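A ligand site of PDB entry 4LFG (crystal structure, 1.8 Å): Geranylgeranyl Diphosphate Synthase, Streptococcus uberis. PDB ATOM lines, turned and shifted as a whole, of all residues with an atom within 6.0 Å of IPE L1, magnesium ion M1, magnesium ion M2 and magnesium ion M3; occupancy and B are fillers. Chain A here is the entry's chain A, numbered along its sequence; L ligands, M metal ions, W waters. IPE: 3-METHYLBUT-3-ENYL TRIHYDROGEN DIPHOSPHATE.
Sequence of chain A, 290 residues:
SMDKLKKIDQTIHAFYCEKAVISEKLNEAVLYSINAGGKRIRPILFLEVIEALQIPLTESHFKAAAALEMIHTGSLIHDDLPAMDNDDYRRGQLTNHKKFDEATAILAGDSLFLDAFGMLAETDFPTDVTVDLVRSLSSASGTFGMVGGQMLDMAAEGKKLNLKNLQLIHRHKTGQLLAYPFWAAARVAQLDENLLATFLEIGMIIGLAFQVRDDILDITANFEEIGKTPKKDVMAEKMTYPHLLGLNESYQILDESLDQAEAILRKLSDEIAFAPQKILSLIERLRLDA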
ATOM      1  N   HIS A  72      34.838 -22.606 -21.855  1.00  0.00           N
ATOM      2  CA  HIS A  72      33.864 -23.033 -22.866  1.00  0.00           C
ATOM      3  C   HIS A  72      33.622 -24.568 -22.794  1.00  0.00           C
ATOM      4  O   HIS A  72      32.463 -25.031 -22.784  1.00  0.00           O
ATOM      5  CB  HIS A  72      34.356 -22.621 -24.245  1.00  0.00           C
ATOM      6  CG  HIS A  72      33.559 -23.221 -25.362  1.00  0.00           C
ATOM      7  ND1 HIS A  72      32.221 -23.011 -25.517  1.00  0.00           N
ATOM      8  CD2 HIS A  72      33.929 -24.063 -26.360  1.00  0.00           C
ATOM      9  CE1 HIS A  72      31.778 -23.683 -26.570  1.00  0.00           C
ATOM     10  NE2 HIS A  72      32.811 -24.320 -27.105  1.00  0.00           N
ATOM     11  N   SER A  75      31.632 -25.629 -19.774  1.00  0.00           N
ATOM     12  CA  SER A  75      30.231 -25.262 -19.952  1.00  0.00           C
ATOM     13  C   SER A  75      29.482 -26.310 -20.784  1.00  0.00           C
ATOM     14  O   SER A  75      28.322 -26.609 -20.485  1.00  0.00           O
ATOM     15  CB  SER A  75      30.091 -23.863 -20.554  1.00  0.00           C
ATOM     16  OG  SER A  75      30.231 -23.835 -21.944  1.00  0.00           O
ATOM     17  N   LEU A  76      30.126 -26.874 -21.785  1.00  0.00           N
ATOM     18  CA  LEU A  76      29.511 -27.926 -22.627  1.00  0.00           C
ATOM     19  C   LEU A  76      29.281 -29.198 -21.844  1.00  0.00           C
ATOM     20  O   LEU A  76      28.225 -29.824 -21.955  1.00  0.00           O
ATOM     21  CB  LEU A  76      30.377 -28.242 -23.851  1.00  0.00           C
ATOM     22  CG  LEU A  76      30.714 -27.106 -24.805  1.00  0.00           C
ATOM     23  CD1 LEU A  76      31.558 -27.622 -25.969  1.00  0.00           C
ATOM     24  CD2 LEU A  76      29.449 -26.443 -25.323  1.00  0.00           C
ATOM     25  N   ASP A  79      26.401 -28.616 -19.637  1.00  0.00           N
ATOM     26  CA  ASP A  79      25.201 -28.396 -20.453  1.00  0.00           C
ATOM     27  C   ASP A  79      24.608 -29.724 -20.927  1.00  0.00           C
ATOM     28  O   ASP A  79      23.387 -29.826 -21.064  1.00  0.00           O
ATOM     29  CB  ASP A  79      25.511 -27.487 -21.634  1.00  0.00           C
ATOM     30  CG  ASP A  79      24.302 -27.284 -22.555  1.00  0.00           C
ATOM     31  OD1 ASP A  79      23.455 -26.424 -22.259  1.00  0.00           O
ATOM     32  OD2 ASP A  79      24.221 -27.957 -23.587  1.00  0.00           O
ATOM     33  N   ASP A  80      25.461 -30.720 -21.182  1.00  0.00           N
ATOM     34  CA  ASP A  80      25.024 -32.038 -21.682  1.00  0.00           C
ATOM     35  C   ASP A  80      24.460 -32.966 -20.623  1.00  0.00           C
ATOM     36  O   ASP A  80      23.854 -33.982 -20.947  1.00  0.00           O
ATOM     37  CB  ASP A  80      26.194 -32.747 -22.383  1.00  0.00           C
ATOM     38  CG  ASP A  80      26.620 -32.073 -23.675  1.00  0.00           C
ATOM     39  OD1 ASP A  80      25.771 -31.453 -24.351  1.00  0.00           O
ATOM     40  OD2 ASP A  80      27.816 -32.189 -24.049  1.00  0.00           O
ATOM     41  N   MET A  84      20.443 -31.280 -17.204  1.00  0.00           N
ATOM     42  CA  MET A  84      20.418 -30.139 -18.097  1.00  0.00           C
ATOM     43  C   MET A  84      19.837 -30.610 -19.437  1.00  0.00           C
ATOM     44  O   MET A  84      18.660 -30.986 -19.469  1.00  0.00           O
ATOM     45  CB  MET A  84      21.832 -29.555 -18.203  1.00  0.00           C
ATOM     46  CG  MET A  84      22.342 -28.999 -16.887  1.00  0.00           C
ATOM     47  SD  MET A  84      21.721 -27.340 -16.575  1.00  0.00           S
ATOM     48  CE  MET A  84      22.532 -26.421 -17.881  1.00  0.00           C
ATOM     49  N   ASP A  85      20.626 -30.635 -20.502  1.00  0.00           N
ATOM     50  CA  ASP A  85      20.091 -30.927 -21.848  1.00  0.00           C
ATOM     51  C   ASP A  85      20.032 -32.432 -22.159  1.00  0.00           C
ATOM     52  O   ASP A  85      19.369 -32.834 -23.138  1.00  0.00           O
ATOM     53  CB  ASP A  85      20.854 -30.169 -22.937  1.00  0.00           C
ATOM     54  CG  ASP A  85      20.622 -28.669 -22.888  1.00  0.00           C
ATOM     55  OD1 ASP A  85      19.660 -28.231 -22.199  1.00  0.00           O
ATOM     56  OD2 ASP A  85      21.375 -27.926 -23.552  1.00  0.00           O
ATOM     57  N   ARG A  90      28.250 -35.275 -28.148  1.00  0.00           N
ATOM     58  CA  ARG A  90      28.860 -33.934 -28.228  1.00  0.00           C
ATOM     59  C   ARG A  90      30.153 -34.098 -29.040  1.00  0.00           C
ATOM     60  O   ARG A  90      30.945 -34.994 -28.780  1.00  0.00           O
ATOM     61  CB  ARG A  90      29.184 -33.421 -26.841  1.00  0.00           C
ATOM     62  CG  ARG A  90      30.094 -32.187 -26.751  1.00  0.00           C
ATOM     63  CD  ARG A  90      29.405 -30.940 -27.251  1.00  0.00           C
ATOM     64  NE  ARG A  90      28.380 -30.453 -26.330  1.00  0.00           N
ATOM     65  CZ  ARG A  90      27.594 -29.415 -26.570  1.00  0.00           C
ATOM     66  NH1 ARG A  90      27.732 -28.696 -27.679  1.00  0.00           N
ATOM     67  NH2 ARG A  90      26.660 -29.090 -25.690  1.00  0.00           N
ATOM     68  N   MET A 146      27.652 -16.359 -18.599  1.00  0.00           N
ATOM     69  CA  MET A 146      27.279 -17.670 -19.098  1.00  0.00           C
ATOM     70  C   MET A 146      26.348 -18.473 -18.171  1.00  0.00           C
ATOM     71  O   MET A 146      25.319 -18.982 -18.627  1.00  0.00           O
ATOM     72  CB  MET A 146      28.541 -18.478 -19.445  1.00  0.00           C
ATOM     73  CG  MET A 146      28.255 -19.862 -20.027  1.00  0.00           C
ATOM     74  SD  MET A 146      28.108 -21.157 -18.794  1.00  0.00           S
ATOM     75  CE  MET A 146      29.781 -21.162 -18.091  1.00  0.00           C
ATOM     76  N   GLN A 150      22.584 -19.706 -18.798  1.00  0.00           N
ATOM     77  CA  GLN A 150      22.192 -21.109 -18.681  1.00  0.00           C
ATOM     78  C   GLN A 150      20.955 -21.293 -17.795  1.00  0.00           C
ATOM     79  O   GLN A 150      20.046 -22.036 -18.160  1.00  0.00           O
ATOM     80  CB  GLN A 150      23.351 -21.976 -18.166  1.00  0.00           C
ATOM     81  CG  GLN A 150      24.442 -22.190 -19.194  1.00  0.00           C
ATOM     82  CD  GLN A 150      23.969 -23.082 -20.334  1.00  0.00           C
ATOM     83  OE1 GLN A 150      23.239 -22.635 -21.216  1.00  0.00           O
ATOM     84  NE2 GLN A 150      24.359 -24.348 -20.298  1.00  0.00           N
ATOM     85  N   ASP A 153      17.892 -20.038 -19.657  1.00  0.00           N
ATOM     86  CA  ASP A 153      17.563 -20.964 -20.743  1.00  0.00           C
ATOM     87  C   ASP A 153      16.704 -22.111 -20.188  1.00  0.00           C
ATOM     88  O   ASP A 153      15.667 -22.480 -20.763  1.00  0.00           O
ATOM     89  CB  ASP A 153      18.880 -21.430 -21.385  1.00  0.00           C
ATOM     90  CG  ASP A 153      18.709 -22.537 -22.414  1.00  0.00           C
ATOM     91  OD1 ASP A 153      18.642 -23.713 -22.019  1.00  0.00           O
ATOM     92  OD2 ASP A 153      18.720 -22.229 -23.630  1.00  0.00           O
ATOM     93  N   MET A 154      17.125 -22.676 -19.067  1.00  0.00           N
ATOM     94  CA  MET A 154      16.357 -23.778 -18.460  1.00  0.00           C
ATOM     95  C   MET A 154      14.995 -23.272 -17.943  1.00  0.00           C
ATOM     96  O   MET A 154      13.994 -23.978 -18.069  1.00  0.00           O
ATOM     97  CB  MET A 154      17.154 -24.494 -17.356  1.00  0.00           C
ATOM     98  CG  MET A 154      18.450 -25.185 -17.823  1.00  0.00           C
ATOM     99  SD  MET A 154      18.297 -26.625 -18.916  1.00  0.00           S
ATOM    100  CE  MET A 154      17.342 -27.776 -17.913  1.00  0.00           C
ATOM    101  N   LYS A 173      24.194 -16.543 -22.251  1.00  0.00           N
ATOM    102  CA  LYS A 173      24.664 -17.920 -22.340  1.00  0.00           C
ATOM    103  C   LYS A 173      25.747 -18.110 -23.396  1.00  0.00           C
ATOM    104  O   LYS A 173      26.600 -18.973 -23.235  1.00  0.00           O
ATOM    105  CB  LYS A 173      23.524 -18.926 -22.547  1.00  0.00           C
ATOM    106  CG  LYS A 173      23.022 -19.105 -23.959  1.00  0.00           C
ATOM    107  CD  LYS A 173      22.097 -20.318 -24.030  1.00  0.00           C
ATOM    108  CE  LYS A 173      21.586 -20.486 -25.445  1.00  0.00           C
ATOM    109  NZ  LYS A 173      20.796 -21.730 -25.629  1.00  0.00           N
ATOM    110  N   THR A 174      25.691 -17.328 -24.466  1.00  0.00           N
ATOM    111  CA  THR A 174      26.627 -17.491 -25.589  1.00  0.00           C
ATOM    112  C   THR A 174      27.383 -16.208 -25.948  1.00  0.00           C
ATOM    113  O   THR A 174      28.577 -16.246 -26.272  1.00  0.00           O
ATOM    114  CB  THR A 174      25.847 -17.999 -26.832  1.00  0.00           C
ATOM    115  OG1 THR A 174      25.315 -19.290 -26.536  1.00  0.00           O
ATOM    116  CG2 THR A 174      26.729 -18.074 -28.087  1.00  0.00           C
ATOM    117  N   GLN A 211      24.732 -17.736 -31.876  1.00  0.00           N
ATOM    118  CA  GLN A 211      23.623 -18.461 -31.288  1.00  0.00           C
ATOM    119  C   GLN A 211      22.432 -18.537 -32.245  1.00  0.00           C
ATOM    120  O   GLN A 211      21.727 -19.549 -32.292  1.00  0.00           O
ATOM    121  CB  GLN A 211      23.201 -17.877 -29.933  1.00  0.00           C
ATOM    122  CG  GLN A 211      22.317 -18.806 -29.095  1.00  0.00           C
ATOM    123  CD  GLN A 211      22.873 -20.209 -28.928  1.00  0.00           C
ATOM    124  OE1 GLN A 211      24.017 -20.403 -28.464  1.00  0.00           O
ATOM    125  NE2 GLN A 211      22.061 -21.204 -29.270  1.00  0.00           N
ATOM    126  N   ASP A 214      23.437 -21.254 -34.385  1.00  0.00           N
ATOM    127  CA  ASP A 214      23.336 -22.554 -33.681  1.00  0.00           C
ATOM    128  C   ASP A 214      21.886 -23.030 -33.623  1.00  0.00           C
ATOM    129  O   ASP A 214      21.599 -24.215 -33.825  1.00  0.00           O
ATOM    130  CB  ASP A 214      23.893 -22.432 -32.264  1.00  0.00           C
ATOM    131  CG  ASP A 214      23.894 -23.767 -31.525  1.00  0.00           C
ATOM    132  OD1 ASP A 214      24.698 -24.630 -31.905  1.00  0.00           O
ATOM    133  OD2 ASP A 214      23.106 -23.920 -30.563  1.00  0.00           O
ATOM    134  N   ASP A 215      20.982 -22.105 -33.328  1.00  0.00           N
ATOM    135  CA  ASP A 215      19.537 -22.382 -33.316  1.00  0.00           C
ATOM    136  C   ASP A 215      19.067 -22.909 -34.687  1.00  0.00           C
ATOM    137  O   ASP A 215      18.291 -23.874 -34.753  1.00  0.00           O
ATOM    138  CB  ASP A 215      18.761 -21.103 -32.984  1.00  0.00           C
ATOM    139  CG  ASP A 215      18.777 -20.738 -31.503  1.00  0.00           C
ATOM    140  OD1 ASP A 215      19.397 -21.433 -30.672  1.00  0.00           O
ATOM    141  OD2 ASP A 215      18.153 -19.701 -31.179  1.00  0.00           O
ATOM    142  N   ASP A 218      20.461 -26.478 -35.307  1.00  0.00           N
ATOM    143  CA  ASP A 218      19.837 -27.517 -34.496  1.00  0.00           C
ATOM    144  C   ASP A 218      18.569 -28.113 -35.117  1.00  0.00           C
ATOM    145  O   ASP A 218      18.200 -29.261 -34.831  1.00  0.00           O
ATOM    146  CB  ASP A 218      19.559 -26.998 -33.094  1.00  0.00           C
ATOM    147  CG  ASP A 218      20.826 -26.866 -32.271  1.00  0.00           C
ATOM    148  OD1 ASP A 218      21.896 -27.316 -32.720  1.00  0.00           O
ATOM    149  OD2 ASP A 218      20.742 -26.302 -31.163  1.00  0.00           O
ATOM    150  N   LYS A 228      26.076 -33.644 -32.493  1.00  0.00           N
ATOM    151  CA  LYS A 228      25.198 -33.688 -31.341  1.00  0.00           C
ATOM    152  C   LYS A 228      23.804 -34.017 -31.876  1.00  0.00           C
ATOM    153  O   LYS A 228      23.595 -34.006 -33.088  1.00  0.00           O
ATOM    154  CB  LYS A 228      25.215 -32.371 -30.555  1.00  0.00           C
ATOM    155  CG  LYS A 228      24.767 -31.141 -31.338  1.00  0.00           C
ATOM    156  CD  LYS A 228      25.370 -29.835 -30.770  1.00  0.00           C
ATOM    157  CE  LYS A 228      24.833 -28.585 -31.483  1.00  0.00           C
ATOM    158  NZ  LYS A 228      25.421 -27.298 -30.976  1.00  0.00           N
ATOM    159  N   ASP A 233      16.243 -28.748 -28.933  1.00  0.00           N
ATOM    160  CA  ASP A 233      15.561 -27.466 -28.643  1.00  0.00           C
ATOM    161  C   ASP A 233      14.044 -27.551 -28.773  1.00  0.00           C
ATOM    162  O   ASP A 233      13.319 -26.995 -27.934  1.00  0.00           O
ATOM    163  CB  ASP A 233      16.029 -26.356 -29.610  1.00  0.00           C
ATOM    164  CG  ASP A 233      17.477 -25.949 -29.400  1.00  0.00           C
ATOM    165  OD1 ASP A 233      18.083 -26.420 -28.402  1.00  0.00           O
ATOM    166  OD2 ASP A 233      18.019 -25.175 -30.237  1.00  0.00           O
ATOM    167  N   LYS A 238      12.490 -25.111 -25.860  1.00  0.00           N
ATOM    168  CA  LYS A 238      13.413 -23.995 -25.624  1.00  0.00           C
ATOM    169  C   LYS A 238      12.990 -22.775 -26.418  1.00  0.00           C
ATOM    170  O   LYS A 238      12.381 -22.899 -27.478  1.00  0.00           O
ATOM    171  CB  LYS A 238      14.819 -24.372 -26.076  1.00  0.00           C
ATOM    172  CG  LYS A 238      15.440 -25.562 -25.366  1.00  0.00           C
ATOM    173  CD  LYS A 238      15.961 -25.188 -23.985  1.00  0.00           C
ATOM    174  CE  LYS A 238      16.819 -26.321 -23.455  1.00  0.00           C
ATOM    175  NZ  LYS A 238      17.470 -26.020 -22.154  1.00  0.00           N
HETATM  176  C1  IPE L   1      24.898 -23.213 -25.649  1.00  0.00           C
HETATM  177  O1  IPE L   1      23.771 -23.959 -25.186  1.00  0.00           O
HETATM  178  C2  IPE L   1      25.476 -22.346 -24.539  1.00  0.00           C
HETATM  179  C3  IPE L   1      26.322 -23.084 -23.524  1.00  0.00           C
HETATM  180  C4  IPE L   1      26.788 -22.413 -22.478  1.00  0.00           C
HETATM  181  C5  IPE L   1      26.656 -24.542 -23.666  1.00  0.00           C
HETATM  182  PA  IPE L   1      22.991 -24.986 -26.121  1.00  0.00           P
HETATM  183  O1A IPE L   1      22.471 -26.048 -25.163  1.00  0.00           O
HETATM  184  O2A IPE L   1      22.032 -24.208 -26.984  1.00  0.00           O
HETATM  185  O3A IPE L   1      24.203 -25.474 -27.070  1.00  0.00           O
HETATM  186  PB  IPE L   1      24.341 -26.932 -27.746  1.00  0.00           P
HETATM  187  O1B IPE L   1      23.295 -27.005 -28.829  1.00  0.00           O
HETATM  188  O2B IPE L   1      24.062 -27.931 -26.643  1.00  0.00           O
HETATM  189  O3B IPE L   1      25.735 -26.932 -28.303  1.00  0.00           O
HETATM  190  C1  IPE L   2      28.517 -24.883 -28.714  1.00  0.00           C
HETATM  191  O1  IPE L   2      29.605 -24.066 -29.110  1.00  0.00           O
HETATM  192  C2  IPE L   2      27.765 -24.162 -27.603  1.00  0.00           C
HETATM  193  C3  IPE L   2      27.276 -22.796 -28.042  1.00  0.00           C
HETATM  194  C4  IPE L   2      27.664 -21.717 -27.401  1.00  0.00           C
HETATM  195  C5  IPE L   2      26.345 -22.674 -29.215  1.00  0.00           C
HETATM  196  PA  IPE L   2      30.454 -24.417 -30.410  1.00  0.00           P
HETATM  197  O1A IPE L   2      29.464 -24.626 -31.538  1.00  0.00           O
HETATM  198  O2A IPE L   2      31.497 -23.354 -30.524  1.00  0.00           O
HETATM  199  O3A IPE L   2      31.039 -25.863 -29.967  1.00  0.00           O
HETATM  200  PB  IPE L   2      32.459 -26.539 -30.282  1.00  0.00           P
HETATM  201  O1B IPE L   2      32.193 -28.022 -30.120  1.00  0.00           O
HETATM  202  O2B IPE L   2      33.354 -25.997 -29.198  1.00  0.00           O
HETATM  203  O3B IPE L   2      32.885 -26.155 -31.664  1.00  0.00           O
HETATM  204 MG    MG M   1      21.711 -25.903 -23.236  1.00  0.00          MG
HETATM  205 MG    MG M   2      22.791 -28.091 -25.056  1.00  0.00          MG
HETATM  206 MG    MG M   3      22.155 -25.604 -29.828  1.00  0.00          MG
HETATM  207  O   HOH W   1      21.226 -28.638 -26.408  1.00  0.00           O
HETATM  208  O   HOH W   2      19.788 -25.392 -24.181  1.00  0.00           O
HETATM  209  O   HOH W   3      23.305 -30.239 -24.889  1.00  0.00           O
HETATM  210  O   HOH W   4      20.448 -26.892 -28.839  1.00  0.00           O
HETATM  211  O   HOH W   5      20.478 -24.161 -29.544  1.00  0.00           O
HETATM  212  O   HOH W   6      20.754 -25.940 -21.403  1.00  0.00           O
HETATM  213  O   HOH W   7      22.093 -23.830 -23.083  1.00  0.00           O
HETATM  214  O   HOH W   8      19.218 -24.589 -26.830  1.00  0.00           O
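The guanidinium group (NH2) of Arg 90 sits close to the side-chain carboxylate (OD2) of Asp 79. OD1 of Asp 79 lies close to NE2 of Gln 150. The side-chain carboxylate (OD1) of Asp 218 lies within salt-bridge range of the side-chain amino group (NZ) of Lys 228 (3.9 Å). The side-chain carboxylate (OD2) of Asp 214 lies close to the side-chain amide nitrogen (NE2) of Gln 211 (3.2 Å). OD1 of Asp 85 is in salt-bridge range of NZ of Lys 238, at 3.1 Å. The guanidinium group (NH2) of Arg 90 is in salt-bridge range of the side-chain carboxylate (OD1) of Asp 80 (2.9 Å). OD2 of Asp 153 is in salt-bridge range of NZ of Lys 173. OE1 of Gln 211 is in hydrogen-bond range of OG1 of Thr 174 (2.6 Å).
O1B of IPE L1 binds magnesium ion M3 (2.1 Å). The side-chain carboxylate (OD2) of Asp 218 binds magnesium ion M3 (2.1 Å). The side-chain carboxylate (OD2) of Asp 214 is bound to magnesium ion M3, 2.1 Å away. Water W5 is bound to magnesium ion M3 (2.2 Å). Water W4 is bound to magnesium ion M3, at 2.4 Å. Magnesium ion M3 has five donor atoms within binding distance.
Residues that only touch magnesium ion M3: Lys 228 (3.9 Å). Three residues have an atom within 4 Å of magnesium ion M3: Asp 214, Asp 218 and Lys 228.
Asp 153 touches magnesium ion M1 (OD1 to MG, 3.96 Å). Within 4 Å of magnesium ion M1: Asp 79, Asp 85 and Asp 153. The nearest printed residue that does not touch magnesium ion M1 is Gln 150 (4.1 Å).
OG of Ser 75 touches C4 of IPE L1, at 3.8 Å. Leu 76 touches IPE L1. Met 146 touches IPE L1 (CG to C4, 3.8 Å). CD of Gln 150 touches C4 of IPE L1 (3.6 Å). Thr 174 touches IPE L1 (OG1 to C2, 3.7 Å). NE2 of Gln 211 touches O2A of IPE L1, at 3.8 Å. Hydrophobic or aromatic side chains within 4 Å of IPE L1: Leu 76 and Met 146. Within 4 Å of IPE L1: Ser 75, Leu 76, Asp 79, Asp 85, Arg 90, Met 146, Gln 150, Lys 173, Thr 174, Gln 211, Asp 214, Asp 218 and Lys 228.
Of the 21 residues printed, 2 come within 4 Å of magnesium ion M2.
Magnesium ion M1 is bound by OD1 of Asp 79 (2.1 Å), water W6 (2.1 Å), OD2 of Asp 85 (2.1 Å), O1A of IPE L1 (2.1 Å), water W7 (2.1 Å) and water W2 (2.2 Å). Magnesium ion M1 has six donor atoms within binding distance.
NZ of Lys 228 lies within salt-bridge range of O3B of IPE L1 (2.7 Å). NH1 of Arg 90 is in salt-bridge range of O3B of IPE L1, 2.7 Å away. O2A of IPE L1 is in salt-bridge range of NZ of Lys 173 (3.1 Å). NE2 of His 72 lies within hydrogen-bond range of O2B of IPE L2, at 2.7 Å.
O2B of IPE L1 is bound to magnesium ion M2, 2.0 Å away. OD2 of Asp 79 is bound to magnesium ion M2 (2.1 Å). Magnesium ion M2 is bound by O1A of IPE L1 (2.1 Å). Magnesium ion M2 is bound by OD2 of Asp 85 (2.1 Å). Magnesium ion M2 is bound by water W1 (2.1 Å). Water W3 is bound to magnesium ion M2, at 2.2 Å. Magnesium ion M2 has six donor atoms within binding distance.
Water W2 lies within hydrogen-bond range of the side-chain carboxylate (OD1) of Asp 153, the side-chain amino group (NZ) of Lys 238 and the side-chain carboxylate (OD1) of Asp 85. Water W7 lies within hydrogen-bond range of OE1 of Gln 150 (2.5 Å) and O1 of IPE L1 (2.7 Å). Water W5 lies within hydrogen-bond range of OD2 of Asp 233, O2A of IPE L1, OD1 of Asp 215 and NE2 of Gln 211. Water W8 lies within hydrogen-bond range of the side-chain carboxylate (OD1) of Asp 233, an oxygen (O2A) of IPE L1 and the side-chain amino group (NZ) of Lys 173.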
